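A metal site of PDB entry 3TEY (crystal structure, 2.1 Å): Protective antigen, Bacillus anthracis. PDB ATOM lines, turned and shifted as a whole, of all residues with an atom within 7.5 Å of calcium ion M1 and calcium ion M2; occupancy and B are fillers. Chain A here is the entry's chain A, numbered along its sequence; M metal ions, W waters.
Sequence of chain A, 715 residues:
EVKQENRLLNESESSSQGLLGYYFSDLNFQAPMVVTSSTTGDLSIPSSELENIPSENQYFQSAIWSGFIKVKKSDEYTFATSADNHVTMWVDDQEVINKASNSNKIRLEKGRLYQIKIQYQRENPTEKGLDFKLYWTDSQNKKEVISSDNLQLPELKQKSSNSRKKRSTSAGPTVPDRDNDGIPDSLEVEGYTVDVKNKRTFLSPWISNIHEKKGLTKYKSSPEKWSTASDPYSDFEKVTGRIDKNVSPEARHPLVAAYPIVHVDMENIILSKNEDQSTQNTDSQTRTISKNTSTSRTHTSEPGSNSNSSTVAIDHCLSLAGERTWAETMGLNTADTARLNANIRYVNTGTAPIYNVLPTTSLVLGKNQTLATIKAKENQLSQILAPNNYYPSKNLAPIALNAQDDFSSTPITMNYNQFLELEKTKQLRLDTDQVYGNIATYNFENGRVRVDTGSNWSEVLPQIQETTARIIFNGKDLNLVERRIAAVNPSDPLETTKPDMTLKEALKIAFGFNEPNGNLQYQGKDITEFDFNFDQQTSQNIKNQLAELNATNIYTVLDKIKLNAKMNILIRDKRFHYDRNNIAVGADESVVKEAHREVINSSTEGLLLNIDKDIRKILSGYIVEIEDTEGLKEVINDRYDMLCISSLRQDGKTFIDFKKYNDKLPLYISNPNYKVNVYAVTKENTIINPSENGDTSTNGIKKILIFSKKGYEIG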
ATOM      1  N   PRO A 176       7.009  13.749  10.192  1.00  0.00           N
ATOM      2  CA  PRO A 176       8.345  14.191  10.613  1.00  0.00           C
ATOM      3  C   PRO A 176       8.308  15.659  11.079  1.00  0.00           C
ATOM      4  O   PRO A 176       8.089  16.563  10.271  1.00  0.00           O
ATOM      5  CB  PRO A 176       9.180  14.060   9.336  1.00  0.00           C
ATOM      6  CG  PRO A 176       8.433  13.038   8.488  1.00  0.00           C
ATOM      7  CD  PRO A 176       6.990  13.245   8.803  1.00  0.00           C
ATOM      8  N   ASP A 177       8.464  15.861  12.382  1.00  0.00           N
ATOM      9  CA  ASP A 177       8.550  17.181  12.988  1.00  0.00           C
ATOM     10  C   ASP A 177       9.574  17.094  14.112  1.00  0.00           C
ATOM     11  O   ASP A 177       9.224  17.163  15.292  1.00  0.00           O
ATOM     12  CB  ASP A 177       7.188  17.620  13.527  1.00  0.00           C
ATOM     13  CG  ASP A 177       7.190  19.064  13.990  1.00  0.00           C
ATOM     14  OD1 ASP A 177       8.093  19.804  13.585  1.00  0.00           O
ATOM     15  OD2 ASP A 177       6.300  19.469  14.765  1.00  0.00           O
ATOM     16  N   ARG A 178      10.846  16.947  13.733  1.00  0.00           N
ATOM     17  CA  ARG A 178      11.914  16.658  14.697  1.00  0.00           C
ATOM     18  C   ARG A 178      12.007  17.676  15.832  1.00  0.00           C
ATOM     19  O   ARG A 178      12.292  17.308  16.968  1.00  0.00           O
ATOM     20  CB  ARG A 178      13.283  16.481  13.997  1.00  0.00           C
ATOM     21  CG  ARG A 178      13.302  15.358  12.943  1.00  0.00           C
ATOM     22  CD  ARG A 178      14.520  15.434  12.001  1.00  0.00           C
ATOM     23  NE  ARG A 178      15.752  14.918  12.607  1.00  0.00           N
ATOM     24  CZ  ARG A 178      16.063  13.628  12.669  1.00  0.00           C
ATOM     25  NH1 ARG A 178      15.239  12.712  12.164  1.00  0.00           N
ATOM     26  NH2 ARG A 178      17.207  13.242  13.236  1.00  0.00           N
ATOM     27  N   ASP A 179      11.759  18.955  15.554  1.00  0.00           N
ATOM     28  CA  ASP A 179      11.905  19.970  16.597  1.00  0.00           C
ATOM     29  C   ASP A 179      10.585  20.314  17.294  1.00  0.00           C
ATOM     30  O   ASP A 179      10.540  21.183  18.173  1.00  0.00           O
ATOM     31  CB  ASP A 179      12.545  21.230  16.035  1.00  0.00           C
ATOM     32  CG  ASP A 179      11.772  21.792  14.867  1.00  0.00           C
ATOM     33  OD1 ASP A 179      10.590  21.452  14.716  1.00  0.00           O
ATOM     34  OD2 ASP A 179      12.349  22.553  14.080  1.00  0.00           O
ATOM     35  N   ASN A 180       9.504  19.656  16.877  1.00  0.00           N
ATOM     36  CA  ASN A 180       8.195  19.844  17.504  1.00  0.00           C
ATOM     37  C   ASN A 180       7.629  21.246  17.405  1.00  0.00           C
ATOM     38  O   ASN A 180       6.866  21.647  18.278  1.00  0.00           O
ATOM     39  CB  ASN A 180       8.219  19.419  18.977  1.00  0.00           C
ATOM     40  CG  ASN A 180       6.828  19.021  19.501  1.00  0.00           C
ATOM     41  OD1 ASN A 180       6.073  18.342  18.797  1.00  0.00           O
ATOM     42  ND2 ASN A 180       6.496  19.453  20.705  1.00  0.00           N
ATOM     43  N   ASP A 181       7.982  22.003  16.361  1.00  0.00           N
ATOM     44  CA  ASP A 181       7.362  23.339  16.251  1.00  0.00           C
ATOM     45  C   ASP A 181       6.025  23.304  15.509  1.00  0.00           C
ATOM     46  O   ASP A 181       5.266  24.273  15.560  1.00  0.00           O
ATOM     47  CB  ASP A 181       8.314  24.416  15.705  1.00  0.00           C
ATOM     48  CG  ASP A 181       8.873  24.074  14.343  1.00  0.00           C
ATOM     49  OD1 ASP A 181       8.264  23.267  13.603  1.00  0.00           O
ATOM     50  OD2 ASP A 181       9.928  24.670  14.002  1.00  0.00           O
ATOM     51  N   GLY A 182       5.735  22.187  14.837  1.00  0.00           N
ATOM     52  CA  GLY A 182       4.482  22.048  14.097  1.00  0.00           C
ATOM     53  C   GLY A 182       4.644  22.126  12.590  1.00  0.00           C
ATOM     54  O   GLY A 182       3.763  21.725  11.832  1.00  0.00           O
ATOM     55  N   ILE A 183       5.788  22.658  12.141  1.00  0.00           N
ATOM     56  CA  ILE A 183       6.088  22.644  10.707  1.00  0.00           C
ATOM     57  C   ILE A 183       6.805  21.333  10.345  1.00  0.00           C
ATOM     58  O   ILE A 183       7.801  20.969  10.947  1.00  0.00           O
ATOM     59  CB  ILE A 183       6.960  23.827  10.298  1.00  0.00           C
ATOM     60  CG1 ILE A 183       6.436  25.127  10.933  1.00  0.00           C
ATOM     61  CG2 ILE A 183       6.988  23.965   8.777  1.00  0.00           C
ATOM     62  CD1 ILE A 183       7.327  26.376  10.633  1.00  0.00           C
ATOM     63  N   PRO A 184       6.269  20.592   9.350  1.00  0.00           N
ATOM     64  CA  PRO A 184       6.952  19.379   8.903  1.00  0.00           C
ATOM     65  C   PRO A 184       8.390  19.619   8.449  1.00  0.00           C
ATOM     66  O   PRO A 184       8.674  20.637   7.792  1.00  0.00           O
ATOM     67  CB  PRO A 184       6.095  18.923   7.706  1.00  0.00           C
ATOM     68  CG  PRO A 184       4.710  19.365   8.066  1.00  0.00           C
ATOM     69  CD  PRO A 184       4.881  20.666   8.850  1.00  0.00           C
ATOM     70  N   ASP A 185       9.286  18.693   8.801  1.00  0.00           N
ATOM     71  CA  ASP A 185      10.670  18.744   8.352  1.00  0.00           C
ATOM     72  C   ASP A 185      10.796  19.207   6.911  1.00  0.00           C
ATOM     73  O   ASP A 185      11.602  20.086   6.590  1.00  0.00           O
ATOM     74  CB  ASP A 185      11.320  17.342   8.431  1.00  0.00           C
ATOM     75  CG  ASP A 185      11.564  16.852   9.851  1.00  0.00           C
ATOM     76  OD1 ASP A 185      10.946  17.368  10.813  1.00  0.00           O
ATOM     77  OD2 ASP A 185      12.381  15.906  10.015  1.00  0.00           O
ATOM     78  N   SER A 186      10.020  18.578   6.021  1.00  0.00           N
ATOM     79  CA  SER A 186      10.196  18.789   4.586  1.00  0.00           C
ATOM     80  C   SER A 186       9.899  20.227   4.148  1.00  0.00           C
ATOM     81  O   SER A 186      10.536  20.752   3.229  1.00  0.00           O
ATOM     82  CB  SER A 186       9.379  17.786   3.761  1.00  0.00           C
ATOM     83  OG  SER A 186       7.982  17.940   3.976  1.00  0.00           O
ATOM     84  N   GLU A 188      10.132  22.987   6.153  1.00  0.00           N
ATOM     85  CA  GLU A 188      11.156  23.875   6.689  1.00  0.00           C
ATOM     86  C   GLU A 188      12.383  23.868   5.791  1.00  0.00           C
ATOM     87  O   GLU A 188      13.020  24.902   5.585  1.00  0.00           O
ATOM     88  CB  GLU A 188      11.535  23.458   8.111  1.00  0.00           C
ATOM     89  CG  GLU A 188      10.395  23.633   9.079  1.00  0.00           C
ATOM     90  CD  GLU A 188      10.886  23.870  10.468  1.00  0.00           C
ATOM     91  OE1 GLU A 188      11.425  24.957  10.725  1.00  0.00           O
ATOM     92  OE2 GLU A 188      10.758  22.974  11.312  1.00  0.00           O
ATOM     93  N   TYR A 192       8.626  27.339   2.440  1.00  0.00           N
ATOM     94  CA  TYR A 192       7.192  27.431   2.630  1.00  0.00           C
ATOM     95  C   TYR A 192       6.704  28.881   2.613  1.00  0.00           C
ATOM     96  O   TYR A 192       7.505  29.821   2.651  1.00  0.00           O
ATOM     97  CB  TYR A 192       6.763  26.720   3.917  1.00  0.00           C
ATOM     98  CG  TYR A 192       7.436  27.216   5.196  1.00  0.00           C
ATOM     99  CD1 TYR A 192       8.713  26.781   5.543  1.00  0.00           C
ATOM    100  CD2 TYR A 192       6.795  28.093   6.051  1.00  0.00           C
ATOM    101  CE1 TYR A 192       9.322  27.222   6.697  1.00  0.00           C
ATOM    102  CE2 TYR A 192       7.410  28.539   7.221  1.00  0.00           C
ATOM    103  CZ  TYR A 192       8.671  28.092   7.545  1.00  0.00           C
ATOM    104  OH  TYR A 192       9.301  28.523   8.694  1.00  0.00           O
ATOM    105  N   SER A 221      13.626  27.395   7.411  1.00  0.00           N
ATOM    106  CA  SER A 221      14.047  27.387   8.816  1.00  0.00           C
ATOM    107  C   SER A 221      14.635  26.016   9.116  1.00  0.00           C
ATOM    108  O   SER A 221      14.491  25.096   8.310  1.00  0.00           O
ATOM    109  CB  SER A 221      12.870  27.712   9.737  1.00  0.00           C
ATOM    110  OG  SER A 221      11.690  27.024   9.336  1.00  0.00           O
ATOM    111  N   SER A 222      15.313  25.850  10.249  1.00  0.00           N
ATOM    112  CA  SER A 222      15.895  24.544  10.546  1.00  0.00           C
ATOM    113  C   SER A 222      14.820  23.571  11.017  1.00  0.00           C
ATOM    114  O   SER A 222      14.061  23.904  11.927  1.00  0.00           O
ATOM    115  CB  SER A 222      16.980  24.617  11.625  1.00  0.00           C
ATOM    116  OG  SER A 222      17.319  23.307  12.055  1.00  0.00           O
ATOM    117  N   PRO A 223      14.777  22.371  10.423  1.00  0.00           N
ATOM    118  CA  PRO A 223      13.841  21.324  10.884  1.00  0.00           C
ATOM    119  C   PRO A 223      14.251  20.791  12.236  1.00  0.00           C
ATOM    120  O   PRO A 223      13.497  20.008  12.838  1.00  0.00           O
ATOM    121  CB  PRO A 223      14.000  20.208   9.835  1.00  0.00           C
ATOM    122  CG  PRO A 223      15.467  20.373   9.346  1.00  0.00           C
ATOM    123  CD  PRO A 223      15.640  21.906   9.321  1.00  0.00           C
ATOM    124  N   GLU A 224      15.430  21.187  12.733  1.00  0.00           N
ATOM    125  CA  GLU A 224      15.891  20.692  14.028  1.00  0.00           C
ATOM    126  C   GLU A 224      16.009  21.729  15.134  1.00  0.00           C
ATOM    127  O   GLU A 224      16.394  21.409  16.262  1.00  0.00           O
ATOM    128  CB  GLU A 224      17.197  19.890  13.880  1.00  0.00           C
ATOM    129  CG  GLU A 224      16.992  18.635  13.040  1.00  0.00           C
ATOM    130  CD  GLU A 224      18.239  17.764  12.923  1.00  0.00           C
ATOM    131  OE1 GLU A 224      19.081  17.774  13.854  1.00  0.00           O
ATOM    132  OE2 GLU A 224      18.363  17.061  11.893  1.00  0.00           O
ATOM    133  N   LYS A 225      15.647  22.977  14.822  1.00  0.00           N
ATOM    134  CA  LYS A 225      15.554  24.019  15.851  1.00  0.00           C
ATOM    135  C   LYS A 225      14.152  24.609  15.957  1.00  0.00           C
ATOM    136  O   LYS A 225      13.643  25.223  15.021  1.00  0.00           O
ATOM    137  CB  LYS A 225      16.547  25.158  15.592  1.00  0.00           C
ATOM    138  CG  LYS A 225      17.986  24.718  15.359  1.00  0.00           C
ATOM    139  CD  LYS A 225      18.903  25.939  15.243  1.00  0.00           C
ATOM    140  CE  LYS A 225      18.754  26.832  16.460  1.00  0.00           C
ATOM    141  NZ  LYS A 225      19.754  27.902  16.444  1.00  0.00           N
ATOM    142  N   TRP A 226      13.566  24.452  17.143  1.00  0.00           N
ATOM    143  CA  TRP A 226      12.235  24.934  17.436  1.00  0.00           C
ATOM    144  C   TRP A 226      12.106  26.433  17.112  1.00  0.00           C
ATOM    145  O   TRP A 226      11.120  26.857  16.489  1.00  0.00           O
ATOM    146  CB  TRP A 226      11.970  24.649  18.922  1.00  0.00           C
ATOM    147  CG  TRP A 226      10.647  25.038  19.439  1.00  0.00           C
ATOM    148  CD1 TRP A 226       9.497  24.307  19.355  1.00  0.00           C
ATOM    149  CD2 TRP A 226      10.321  26.219  20.176  1.00  0.00           C
ATOM    150  NE1 TRP A 226       8.476  24.968  19.988  1.00  0.00           N
ATOM    151  CE2 TRP A 226       8.955  26.148  20.500  1.00  0.00           C
ATOM    152  CE3 TRP A 226      11.062  27.347  20.590  1.00  0.00           C
ATOM    153  CZ2 TRP A 226       8.306  27.154  21.212  1.00  0.00           C
ATOM    154  CZ3 TRP A 226      10.403  28.345  21.295  1.00  0.00           C
ATOM    155  CH2 TRP A 226       9.037  28.240  21.597  1.00  0.00           C
ATOM    156  N   SER A 227      13.111  27.220  17.516  1.00  0.00           N
ATOM    157  CA  SER A 227      13.299  28.603  17.051  1.00  0.00           C
ATOM    158  C   SER A 227      14.623  28.640  16.277  1.00  0.00           C
ATOM    159  O   SER A 227      15.705  28.498  16.863  1.00  0.00           O
ATOM    160  CB  SER A 227      13.380  29.604  18.209  1.00  0.00           C
ATOM    161  OG  SER A 227      13.702  30.936  17.761  1.00  0.00           O
ATOM    162  N   THR A 228      14.550  28.824  14.977  1.00  0.00           N
ATOM    163  CA  THR A 228      15.769  28.801  14.184  1.00  0.00           C
ATOM    164  C   THR A 228      16.760  29.912  14.586  1.00  0.00           C
ATOM    165  O   THR A 228      17.972  29.725  14.475  1.00  0.00           O
ATOM    166  CB  THR A 228      15.463  28.781  12.683  1.00  0.00           C
ATOM    167  OG1 THR A 228      14.760  27.565  12.382  1.00  0.00           O
ATOM    168  CG2 THR A 228      16.754  28.856  11.840  1.00  0.00           C
ATOM    169  N   SER A 234       8.795  30.175  18.596  1.00  0.00           N
ATOM    170  CA  SER A 234       9.063  29.104  17.632  1.00  0.00           C
ATOM    171  C   SER A 234       8.884  29.571  16.198  1.00  0.00           C
ATOM    172  O   SER A 234       8.209  30.562  15.905  1.00  0.00           O
ATOM    173  CB  SER A 234       8.152  27.885  17.887  1.00  0.00           C
ATOM    174  OG  SER A 234       6.959  27.983  17.126  1.00  0.00           O
ATOM    175  N   ASP A 235       9.466  28.809  15.276  1.00  0.00           N
ATOM    176  CA  ASP A 235       9.313  29.137  13.865  1.00  0.00           C
ATOM    177  C   ASP A 235       7.844  29.194  13.460  1.00  0.00           C
ATOM    178  O   ASP A 235       7.419  30.043  12.648  1.00  0.00           O
ATOM    179  CB  ASP A 235      10.088  28.112  13.030  1.00  0.00           C
ATOM    180  CG  ASP A 235      11.599  28.114  13.324  1.00  0.00           C
ATOM    181  OD1 ASP A 235      12.159  29.161  13.771  1.00  0.00           O
ATOM    182  OD2 ASP A 235      12.214  27.051  13.068  1.00  0.00           O
ATOM    183  N   PHE A 236       7.056  28.256  13.997  1.00  0.00           N
ATOM    184  CA  PHE A 236       5.606  28.184  13.763  1.00  0.00           C
ATOM    185  C   PHE A 236       4.833  29.344  14.404  1.00  0.00           C
ATOM    186  O   PHE A 236       3.959  29.965  13.769  1.00  0.00           O
ATOM    187  CB  PHE A 236       5.087  26.837  14.269  1.00  0.00           C
ATOM    188  CG  PHE A 236       3.642  26.602  14.040  1.00  0.00           C
ATOM    189  CD1 PHE A 236       3.180  26.253  12.774  1.00  0.00           C
ATOM    190  CD2 PHE A 236       2.742  26.654  15.081  1.00  0.00           C
ATOM    191  CE1 PHE A 236       1.824  25.987  12.550  1.00  0.00           C
ATOM    192  CE2 PHE A 236       1.383  26.385  14.866  1.00  0.00           C
ATOM    193  CZ  PHE A 236       0.935  26.046  13.598  1.00  0.00           C
ATOM    194  N   PRO A 254      11.355  33.626  10.656  1.00  0.00           N
ATOM    195  CA  PRO A 254      12.050  32.625  11.465  1.00  0.00           C
ATOM    196  C   PRO A 254      13.580  32.785  11.467  1.00  0.00           C
ATOM    197  O   PRO A 254      14.249  32.204  12.334  1.00  0.00           O
ATOM    198  CB  PRO A 254      11.680  31.299  10.769  1.00  0.00           C
ATOM    199  CG  PRO A 254      10.436  31.580   9.989  1.00  0.00           C
ATOM    200  CD  PRO A 254      10.534  33.037   9.578  1.00  0.00           C
HETATM  201 CA    CA M   1      12.080  24.660  13.123  1.00  0.00          CA
HETATM  202 CA    CA M   2       9.464  21.424  12.590  1.00  0.00          CA
HETATM  203  O   HOH W   1      11.206  19.601  11.771  1.00  0.00           O
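The backbone NH of Asp 179 lies close to the backbone carbonyl oxygen of Pro 223 (3.4 Å). OD2 of Asp 177 is in hydrogen-bond range of N of Gly 182 (2.8 Å). O of Glu 188 lies within hydrogen-bond range of N of Ser 221 (3.1 Å). OD1 of Asp 235 lies within hydrogen-bond range of N of Thr 228, 2.7 Å away. The backbone NH (N) of Asp 235 sits at hydrogen-bond distance from the backbone carbonyl oxygen (O) of Trp 226 (2.8 Å). The side-chain hydroxyl (OG) of Ser 222 sits at hydrogen-bond distance from the backbone NH (N) of Lys 225 (3.2 Å). OG1 of Thr 228 sits at hydrogen-bond distance from N of Ser 222, 2.8 Å away. The side-chain amino group (NZ) of Lys 225 is in hydrogen-bond range of the backbone carbonyl oxygen (O) of Thr 228 (3.2 Å).
The nearest printed residue that does not touch calcium ion M2 is Pro 223 (4.3 Å).
Calcium ion M1 is bound by the side-chain carboxylate (OD2) of Asp 181, the side-chain carboxylate (OD2) of Asp 179, the side-chain carboxylate (OD2) of Asp 235, the backbone carbonyl oxygen (O) of Ser 222, the side-chain carboxylate (OE1) of Glu 188, the backbone carbonyl oxygen (O) of Lys 225 and the side-chain carboxylate (OE2) of Glu 188.
OD1 of Asp 177 binds calcium ion M2, at 2.3 Å. The backbone carbonyl oxygen (O) of Ile 183 is bound to calcium ion M2 (2.4 Å). Calcium ion M2 is bound by the side-chain carboxylate (OE2) of Glu 188, at 2.4 Å. OD1 of Asp 179 is bound to calcium ion M2. OD1 of Asp 181 binds calcium ion M2 (2.4 Å). Calcium ion M2 is bound by water W1 (2.7 Å).
Water W1 lies within hydrogen-bond range of the side-chain carboxylate (OD1) of Asp 185 (2.4 Å), the backbone carbonyl oxygen (O) of Pro 223 (2.6 Å) and the backbone NH (N) of Arg 178 (3.3 Å).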
